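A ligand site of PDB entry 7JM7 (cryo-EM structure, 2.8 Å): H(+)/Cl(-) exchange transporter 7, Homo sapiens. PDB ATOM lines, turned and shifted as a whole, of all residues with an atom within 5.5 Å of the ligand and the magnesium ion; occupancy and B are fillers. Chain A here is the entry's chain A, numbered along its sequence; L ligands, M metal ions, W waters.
The magnesium ion is bound by O4 of the ligand and OE2 of Glu 95.
The magnesium ion has two donor atoms within binding distance.
OE2 of Glu 95 sits close to ND2 of Asn 659.
N of Ser 632 sits at hydrogen-bond distance from O of Leu 781 (3.1 Å).
OG of Ser 96 lies within hydrogen-bond range of NE of Arg 784.
The side-chain carboxylate (OD2) of Asp 786 sits at hydrogen-bond distance from the backbone NH (N) of Thr 783 (3.2 Å).
The side-chain hydroxyl (OG) of Ser 632 is in hydrogen-bond range of the side-chain carboxylate (OD1) of Asp 786.
NE2 of His 658 sits at hydrogen-bond distance from OG of Ser 656.
OE2 of Glu 95 lies close to NH1 of Arg 767, 3.1 Å away.
Of the 23 residues printed, 1 comes within 4 Å of the magnesium ion.
Water W1 bridges O3 of the ligand (2.7 Å) and O of Tyr 94 (2.8 Å).
Residues that only touch the ligand: Pro 634, Val 635, Asn 659, Leu 781, Thr 783 and Arg 784.
Hydrophobic or aromatic side chains within 4 Å of the ligand: Val 635, His 658, His 768 and Leu 781.
Within 4 Å of the ligand: Glu 95, Ser 96, Ser 632, Pro 634, Val 635, Thr 636, Asn 657, His 658, Asn 659, Gly 660, Arg 767, His 768, Leu 781, Thr 783, Arg 784, Lys 785 and Asp 786.
The side-chain carboxylate of Asp 786 lies within hydrogen-bond range of an oxygen (O13) of the ligand (3.1 Å).
O of Thr 636 sits at hydrogen-bond distance from N3 of the ligand, at 3.4 Å.
A ring nitrogen (NE2) of His 768 is in hydrogen-bond range of an oxygen (O5) of the ligand, 3.2 Å away.
The backbone carbonyl oxygen of Asn 657 sits close to an oxygen (O7) of the ligand (2.6 Å).
An oxygen (O3) of the ligand is in hydrogen-bond range of the side-chain hydroxyl of Ser 96, at 2.6 Å.
N of Thr 636 is in hydrogen-bond range of N4 of the ligand (3.0 Å).
The side-chain amino group (NZ) of Lys 785 lies within salt-bridge range of an oxygen (O8) of the ligand, 2.5 Å away.
O1 of the ligand lies within hydrogen-bond range of N of Ser 96.
The side-chain hydroxyl of Ser 632 sits at hydrogen-bond distance from an oxygen (O13) of the ligand.
O7 of the ligand lies within hydrogen-bond range of ND1 of His 658 (2.9 Å).
The guanidinium group of Arg 767 is in salt-bridge range of an oxygen (O1) of the ligand (2.9 Å).
The backbone carbonyl oxygen of Gly 660 lies within hydrogen-bond range of a nitrogen (N3) of the ligand (3.3 Å).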
ATOM      1  N   LEU A  92      17.181 -15.820 -26.686  1.00  0.00           N
ATOM      2  CA  LEU A  92      17.754 -17.138 -26.879  1.00  0.00           C
ATOM      3  C   LEU A  92      18.660 -17.573 -25.738  1.00  0.00           C
ATOM      4  O   LEU A  92      19.131 -18.715 -25.730  1.00  0.00           O
ATOM      5  CB  LEU A  92      18.549 -17.178 -28.189  1.00  0.00           C
ATOM      6  CG  LEU A  92      17.704 -17.415 -29.441  1.00  0.00           C
ATOM      7  CD1 LEU A  92      16.870 -16.182 -29.775  1.00  0.00           C
ATOM      8  CD2 LEU A  92      18.584 -17.800 -30.623  1.00  0.00           C
ATOM      9  N   TYR A  94      17.449 -17.808 -22.759  1.00  0.00           N
ATOM     10  CA  TYR A  94      16.511 -18.457 -21.850  1.00  0.00           C
ATOM     11  C   TYR A  94      16.292 -19.890 -22.327  1.00  0.00           C
ATOM     12  O   TYR A  94      15.595 -20.117 -23.322  1.00  0.00           O
ATOM     13  CB  TYR A  94      15.194 -17.687 -21.803  1.00  0.00           C
ATOM     14  CG  TYR A  94      15.332 -16.260 -21.330  1.00  0.00           C
ATOM     15  CD1 TYR A  94      15.035 -15.201 -22.167  1.00  0.00           C
ATOM     16  CD2 TYR A  94      15.755 -15.981 -20.037  1.00  0.00           C
ATOM     17  CE1 TYR A  94      15.159 -13.895 -21.741  1.00  0.00           C
ATOM     18  CE2 TYR A  94      15.875 -14.683 -19.597  1.00  0.00           C
ATOM     19  CZ  TYR A  94      15.580 -13.645 -20.457  1.00  0.00           C
ATOM     20  OH  TYR A  94      15.698 -12.346 -20.030  1.00  0.00           O
ATOM     21  N   GLU A  95      16.882 -20.850 -21.624  1.00  0.00           N
ATOM     22  CA  GLU A  95      16.737 -22.248 -21.970  1.00  0.00           C
ATOM     23  C   GLU A  95      15.417 -22.774 -21.388  1.00  0.00           C
ATOM     24  O   GLU A  95      14.594 -22.018 -20.873  1.00  0.00           O
ATOM     25  CB  GLU A  95      17.936 -23.052 -21.477  1.00  0.00           C
ATOM     26  CG  GLU A  95      19.251 -22.645 -22.115  1.00  0.00           C
ATOM     27  CD  GLU A  95      19.479 -23.292 -23.469  1.00  0.00           C
ATOM     28  OE1 GLU A  95      20.555 -23.092 -24.051  1.00  0.00           O
ATOM     29  OE2 GLU A  95      18.568 -24.001 -23.942  1.00  0.00           O
ATOM     30  N   SER A  96      15.212 -24.084 -21.469  1.00  0.00           N
ATOM     31  CA  SER A  96      13.993 -24.712 -20.995  1.00  0.00           C
ATOM     32  C   SER A  96      14.324 -25.785 -19.956  1.00  0.00           C
ATOM     33  O   SER A  96      15.465 -26.240 -19.836  1.00  0.00           O
ATOM     34  CB  SER A  96      13.214 -25.353 -22.155  1.00  0.00           C
ATOM     35  OG  SER A  96      12.761 -24.365 -23.062  1.00  0.00           O
ATOM     36  N   SER A 632       9.720 -26.685 -37.287  1.00  0.00           N
ATOM     37  CA  SER A 632      10.873 -26.079 -37.943  1.00  0.00           C
ATOM     38  C   SER A 632      11.575 -27.126 -38.803  1.00  0.00           C
ATOM     39  O   SER A 632      11.825 -28.245 -38.351  1.00  0.00           O
ATOM     40  CB  SER A 632      11.844 -25.507 -36.910  1.00  0.00           C
ATOM     41  OG  SER A 632      11.325 -24.321 -36.345  1.00  0.00           O
ATOM     42  N   PRO A 634      14.745 -27.563 -42.114  1.00  0.00           N
ATOM     43  CA  PRO A 634      14.978 -29.006 -41.925  1.00  0.00           C
ATOM     44  C   PRO A 634      15.441 -29.341 -40.517  1.00  0.00           C
ATOM     45  O   PRO A 634      15.941 -28.460 -39.817  1.00  0.00           O
ATOM     46  CB  PRO A 634      16.062 -29.326 -42.953  1.00  0.00           C
ATOM     47  CG  PRO A 634      16.815 -28.056 -43.094  1.00  0.00           C
ATOM     48  CD  PRO A 634      15.817 -26.944 -42.918  1.00  0.00           C
ATOM     49  N   VAL A 635      15.272 -30.592 -40.108  1.00  0.00           N
ATOM     50  CA  VAL A 635      15.627 -31.044 -38.763  1.00  0.00           C
ATOM     51  C   VAL A 635      17.007 -31.675 -38.802  1.00  0.00           C
ATOM     52  O   VAL A 635      17.349 -32.408 -39.736  1.00  0.00           O
ATOM     53  CB  VAL A 635      14.586 -32.033 -38.213  1.00  0.00           C
ATOM     54  CG1 VAL A 635      14.990 -32.528 -36.838  1.00  0.00           C
ATOM     55  CG2 VAL A 635      13.231 -31.378 -38.142  1.00  0.00           C
ATOM     56  N   THR A 636      17.807 -31.388 -37.776  1.00  0.00           N
ATOM     57  CA  THR A 636      19.107 -32.018 -37.593  1.00  0.00           C
ATOM     58  C   THR A 636      18.909 -33.283 -36.764  1.00  0.00           C
ATOM     59  O   THR A 636      18.554 -33.203 -35.582  1.00  0.00           O
ATOM     60  CB  THR A 636      20.085 -31.059 -36.917  1.00  0.00           C
ATOM     61  OG1 THR A 636      20.047 -29.788 -37.575  1.00  0.00           O
ATOM     62  CG2 THR A 636      21.498 -31.613 -36.973  1.00  0.00           C
ATOM     63  N   SER A 656      23.837 -22.205 -34.386  1.00  0.00           N
ATOM     64  CA  SER A 656      22.785 -22.346 -33.392  1.00  0.00           C
ATOM     65  C   SER A 656      23.193 -23.432 -32.400  1.00  0.00           C
ATOM     66  O   SER A 656      24.047 -24.268 -32.701  1.00  0.00           O
ATOM     67  CB  SER A 656      21.439 -22.667 -34.033  1.00  0.00           C
ATOM     68  OG  SER A 656      21.479 -23.932 -34.683  1.00  0.00           O
ATOM     69  N   ASN A 657      22.559 -23.406 -31.237  1.00  0.00           N
ATOM     70  CA  ASN A 657      22.838 -24.350 -30.157  1.00  0.00           C
ATOM     71  C   ASN A 657      21.543 -25.083 -29.825  1.00  0.00           C
ATOM     72  O   ASN A 657      20.720 -24.580 -29.049  1.00  0.00           O
ATOM     73  CB  ASN A 657      23.411 -23.653 -28.940  1.00  0.00           C
ATOM     74  CG  ASN A 657      23.457 -24.541 -27.716  1.00  0.00           C
ATOM     75  OD1 ASN A 657      23.530 -25.763 -27.833  1.00  0.00           O
ATOM     76  ND2 ASN A 657      23.427 -23.934 -26.541  1.00  0.00           N
ATOM     77  N   HIS A 658      21.369 -26.265 -30.400  1.00  0.00           N
ATOM     78  CA  HIS A 658      20.210 -27.116 -30.142  1.00  0.00           C
ATOM     79  C   HIS A 658      20.589 -28.148 -29.083  1.00  0.00           C
ATOM     80  O   HIS A 658      21.618 -28.815 -29.203  1.00  0.00           O
ATOM     81  CB  HIS A 658      19.744 -27.815 -31.413  1.00  0.00           C
ATOM     82  CG  HIS A 658      19.386 -26.869 -32.525  1.00  0.00           C
ATOM     83  ND1 HIS A 658      18.659 -25.722 -32.322  1.00  0.00           N
ATOM     84  CD2 HIS A 658      19.657 -26.919 -33.854  1.00  0.00           C
ATOM     85  CE1 HIS A 658      18.494 -25.100 -33.469  1.00  0.00           C
ATOM     86  NE2 HIS A 658      19.092 -25.804 -34.416  1.00  0.00           N
ATOM     87  N   ASN A 659      19.744 -28.277 -28.062  1.00  0.00           N
ATOM     88  CA  ASN A 659      19.994 -29.187 -26.952  1.00  0.00           C
ATOM     89  C   ASN A 659      19.193 -30.478 -27.048  1.00  0.00           C
ATOM     90  O   ASN A 659      19.130 -31.230 -26.075  1.00  0.00           O
ATOM     91  CB  ASN A 659      19.702 -28.495 -25.625  1.00  0.00           C
ATOM     92  CG  ASN A 659      20.745 -27.443 -25.278  1.00  0.00           C
ATOM     93  OD1 ASN A 659      21.732 -27.739 -24.605  1.00  0.00           O
ATOM     94  ND2 ASN A 659      20.519 -26.221 -25.729  1.00  0.00           N
ATOM     95  N   GLY A 660      18.579 -30.742 -28.195  1.00  0.00           N
ATOM     96  CA  GLY A 660      17.834 -31.978 -28.395  1.00  0.00           C
ATOM     97  C   GLY A 660      17.795 -32.393 -29.849  1.00  0.00           C
ATOM     98  O   GLY A 660      17.499 -31.582 -30.729  1.00  0.00           O
ATOM     99  N   PHE A 661      18.094 -33.666 -30.115  1.00  0.00           N
ATOM    100  CA  PHE A 661      18.177 -34.183 -31.464  1.00  0.00           C
ATOM    101  C   PHE A 661      17.378 -35.474 -31.546  1.00  0.00           C
ATOM    102  O   PHE A 661      17.589 -36.381 -30.732  1.00  0.00           O
ATOM    103  CB  PHE A 661      19.639 -34.433 -31.862  1.00  0.00           C
ATOM    104  CG  PHE A 661      20.571 -33.312 -31.501  1.00  0.00           C
ATOM    105  CD1 PHE A 661      20.947 -32.383 -32.447  1.00  0.00           C
ATOM    106  CD2 PHE A 661      21.067 -33.191 -30.212  1.00  0.00           C
ATOM    107  CE1 PHE A 661      21.792 -31.353 -32.129  1.00  0.00           C
ATOM    108  CE2 PHE A 661      21.915 -32.162 -29.880  1.00  0.00           C
ATOM    109  CZ  PHE A 661      22.281 -31.240 -30.839  1.00  0.00           C
ATOM    110  N   PRO A 662      16.451 -35.595 -32.497  1.00  0.00           N
ATOM    111  CA  PRO A 662      15.751 -36.873 -32.681  1.00  0.00           C
ATOM    112  C   PRO A 662      16.608 -37.858 -33.442  1.00  0.00           C
ATOM    113  O   PRO A 662      17.314 -37.511 -34.396  1.00  0.00           O
ATOM    114  CB  PRO A 662      14.499 -36.477 -33.477  1.00  0.00           C
ATOM    115  CG  PRO A 662      14.894 -35.265 -34.223  1.00  0.00           C
ATOM    116  CD  PRO A 662      15.930 -34.553 -33.400  1.00  0.00           C
ATOM    117  N   ARG A 767       9.695 -30.383 -23.776  1.00  0.00           N
ATOM    118  CA  ARG A 767      10.695 -29.485 -24.351  1.00  0.00           C
ATOM    119  C   ARG A 767      10.837 -29.662 -25.853  1.00  0.00           C
ATOM    120  O   ARG A 767      10.936 -28.664 -26.573  1.00  0.00           O
ATOM    121  CB  ARG A 767      12.052 -29.723 -23.686  1.00  0.00           C
ATOM    122  CG  ARG A 767      13.057 -28.636 -23.953  1.00  0.00           C
ATOM    123  CD  ARG A 767      14.414 -28.976 -23.388  1.00  0.00           C
ATOM    124  NE  ARG A 767      15.365 -27.881 -23.584  1.00  0.00           N
ATOM    125  CZ  ARG A 767      16.607 -27.883 -23.119  1.00  0.00           C
ATOM    126  NH1 ARG A 767      17.402 -26.851 -23.342  1.00  0.00           N
ATOM    127  NH2 ARG A 767      17.063 -28.926 -22.434  1.00  0.00           N
ATOM    128  N   HIS A 768      10.836 -30.902 -26.340  1.00  0.00           N
ATOM    129  CA  HIS A 768      10.912 -31.197 -27.754  1.00  0.00           C
ATOM    130  C   HIS A 768       9.749 -32.095 -28.138  1.00  0.00           C
ATOM    131  O   HIS A 768       9.497 -33.107 -27.471  1.00  0.00           O
ATOM    132  CB  HIS A 768      12.237 -31.871 -28.117  1.00  0.00           C
ATOM    133  CG  HIS A 768      13.441 -31.085 -27.728  1.00  0.00           C
ATOM    134  ND1 HIS A 768      14.168 -31.343 -26.586  1.00  0.00           N
ATOM    135  CD2 HIS A 768      14.061 -30.045 -28.339  1.00  0.00           C
ATOM    136  CE1 HIS A 768      15.168 -30.491 -26.496  1.00  0.00           C
ATOM    137  NE2 HIS A 768      15.130 -29.694 -27.545  1.00  0.00           N
ATOM    138  N   LEU A 781      10.395 -30.498 -35.804  1.00  0.00           N
ATOM    139  CA  LEU A 781      10.517 -30.421 -34.360  1.00  0.00           C
ATOM    140  C   LEU A 781       9.818 -29.169 -33.866  1.00  0.00           C
ATOM    141  O   LEU A 781       9.781 -28.142 -34.546  1.00  0.00           O
ATOM    142  CB  LEU A 781      11.990 -30.414 -33.918  1.00  0.00           C
ATOM    143  CG  LEU A 781      12.283 -30.997 -32.537  1.00  0.00           C
ATOM    144  CD1 LEU A 781      11.913 -32.462 -32.487  1.00  0.00           C
ATOM    145  CD2 LEU A 781      13.735 -30.802 -32.195  1.00  0.00           C
ATOM    146  N   VAL A 782       9.252 -29.259 -32.660  1.00  0.00           N
ATOM    147  CA  VAL A 782       8.518 -28.164 -32.044  1.00  0.00           C
ATOM    148  C   VAL A 782       9.061 -27.929 -30.643  1.00  0.00           C
ATOM    149  O   VAL A 782       9.196 -28.880 -29.858  1.00  0.00           O
ATOM    150  CB  VAL A 782       7.001 -28.458 -32.006  1.00  0.00           C
ATOM    151  CG1 VAL A 782       6.308 -27.539 -31.011  1.00  0.00           C
ATOM    152  CG2 VAL A 782       6.404 -28.294 -33.372  1.00  0.00           C
ATOM    153  N   THR A 783       9.381 -26.669 -30.345  1.00  0.00           N
ATOM    154  CA  THR A 783       9.812 -26.251 -29.017  1.00  0.00           C
ATOM    155  C   THR A 783       8.915 -25.107 -28.564  1.00  0.00           C
ATOM    156  O   THR A 783       8.039 -24.647 -29.297  1.00  0.00           O
ATOM    157  CB  THR A 783      11.288 -25.813 -29.029  1.00  0.00           C
ATOM    158  OG1 THR A 783      11.423 -24.580 -29.744  1.00  0.00           O
ATOM    159  CG2 THR A 783      12.167 -26.871 -29.669  1.00  0.00           C
ATOM    160  N   ARG A 784       9.132 -24.649 -27.330  1.00  0.00           N
ATOM    161  CA  ARG A 784       8.273 -23.610 -26.769  1.00  0.00           C
ATOM    162  C   ARG A 784       8.325 -22.327 -27.592  1.00  0.00           C
ATOM    163  O   ARG A 784       7.318 -21.599 -27.654  1.00  0.00           O
ATOM    164  CB  ARG A 784       8.677 -23.330 -25.326  1.00  0.00           C
ATOM    165  CG  ARG A 784      10.051 -22.720 -25.160  1.00  0.00           C
ATOM    166  CD  ARG A 784      10.319 -22.333 -23.710  1.00  0.00           C
ATOM    167  NE  ARG A 784       9.836 -23.342 -22.773  1.00  0.00           N
ATOM    168  CZ  ARG A 784       8.785 -23.189 -21.965  1.00  0.00           C
ATOM    169  NH1 ARG A 784       8.082 -22.069 -21.943  1.00  0.00           N
ATOM    170  NH2 ARG A 784       8.441 -24.187 -21.161  1.00  0.00           N
ATOM    171  N   LYS A 785       9.449 -22.027 -28.223  1.00  0.00           N
ATOM    172  CA  LYS A 785       9.562 -20.798 -29.005  1.00  0.00           C
ATOM    173  C   LYS A 785       8.678 -20.838 -30.237  1.00  0.00           C
ATOM    174  O   LYS A 785       8.185 -19.788 -30.673  1.00  0.00           O
ATOM    175  CB  LYS A 785      11.017 -20.557 -29.387  1.00  0.00           C
ATOM    176  CG  LYS A 785      11.788 -19.746 -28.361  1.00  0.00           C
ATOM    177  CD  LYS A 785      13.204 -19.452 -28.826  1.00  0.00           C
ATOM    178  CE  LYS A 785      14.100 -20.656 -28.628  1.00  0.00           C
ATOM    179  NZ  LYS A 785      15.531 -20.323 -28.854  1.00  0.00           N
ATOM    180  N   ASP A 786       8.478 -22.011 -30.826  1.00  0.00           N
ATOM    181  CA  ASP A 786       7.562 -22.130 -31.954  1.00  0.00           C
ATOM    182  C   ASP A 786       6.137 -21.788 -31.544  1.00  0.00           C
ATOM    183  O   ASP A 786       5.416 -21.115 -32.285  1.00  0.00           O
ATOM    184  CB  ASP A 786       7.619 -23.541 -32.529  1.00  0.00           C
ATOM    185  CG  ASP A 786       8.955 -23.859 -33.157  1.00  0.00           C
ATOM    186  OD1 ASP A 786       9.629 -22.934 -33.634  1.00  0.00           O
ATOM    187  OD2 ASP A 786       9.331 -25.050 -33.159  1.00  0.00           O
HETATM  188  P1  LIG L   1      14.435 -24.870 -25.449  1.00  0.00           P
HETATM  189  O1  LIG L   1      15.721 -24.836 -24.672  1.00  0.00           O
HETATM  190  O2  LIG L   1      13.628 -26.143 -25.303  1.00  0.00           O
HETATM  191  O3  LIG L   1      13.614 -23.605 -25.348  1.00  0.00           O
HETATM  192  P2  LIG L   1      16.371 -25.351 -27.407  1.00  0.00           P
HETATM  193  O4  LIG L   1      17.374 -24.379 -26.838  1.00  0.00           O
HETATM  194  O5  LIG L   1      16.498 -26.834 -27.152  1.00  0.00           O
HETATM  195  O6  LIG L   1      14.897 -24.876 -26.993  1.00  0.00           O
HETATM  196  P3  LIG L   1      16.952 -23.806 -29.642  1.00  0.00           P
HETATM  197  O7  LIG L   1      18.389 -24.081 -30.000  1.00  0.00           O
HETATM  198  O8  LIG L   1      16.581 -22.631 -28.771  1.00  0.00           O
HETATM  199  O9  LIG L   1      16.303 -25.124 -28.998  1.00  0.00           O
HETATM  200  O10 LIG L   1      16.105 -23.693 -31.005  1.00  0.00           O
HETATM  201  C1  LIG L   1      16.063 -22.490 -31.760  1.00  0.00           C
HETATM  202  C2  LIG L   1      15.216 -22.777 -32.986  1.00  0.00           C
HETATM  203  O11 LIG L   1      15.748 -23.922 -33.654  1.00  0.00           O
HETATM  204  C3  LIG L   1      13.777 -23.091 -32.604  1.00  0.00           C
HETATM  205  O12 LIG L   1      12.876 -22.238 -33.323  1.00  0.00           O
HETATM  206  C4  LIG L   1      13.563 -24.552 -32.968  1.00  0.00           C
HETATM  207  O13 LIG L   1      12.337 -24.719 -33.672  1.00  0.00           O
HETATM  208  C5  LIG L   1      14.752 -24.936 -33.835  1.00  0.00           C
HETATM  209  N1  LIG L   1      15.315 -26.270 -33.503  1.00  0.00           N
HETATM  210  C6  LIG L   1      15.498 -26.814 -32.284  1.00  0.00           C
HETATM  211  N2  LIG L   1      16.029 -28.060 -32.376  1.00  0.00           N
HETATM  212  C7  LIG L   1      16.208 -28.326 -33.681  1.00  0.00           C
HETATM  213  C8  LIG L   1      16.730 -29.454 -34.483  1.00  0.00           C
HETATM  214  N3  LIG L   1      17.188 -30.571 -33.890  1.00  0.00           N
HETATM  215  N4  LIG L   1      16.735 -29.315 -35.827  1.00  0.00           N
HETATM  216  C9  LIG L   1      16.284 -28.208 -36.437  1.00  0.00           C
HETATM  217  N5  LIG L   1      15.798 -27.150 -35.764  1.00  0.00           N
HETATM  218  C10 LIG L   1      15.734 -27.146 -34.412  1.00  0.00           C
HETATM  219 MG    MG M   1      18.255 -22.825 -26.047  1.00  0.00          MG
HETATM  220  O   HOH W   1      13.218 -21.023 -24.577  1.00  0.00           O
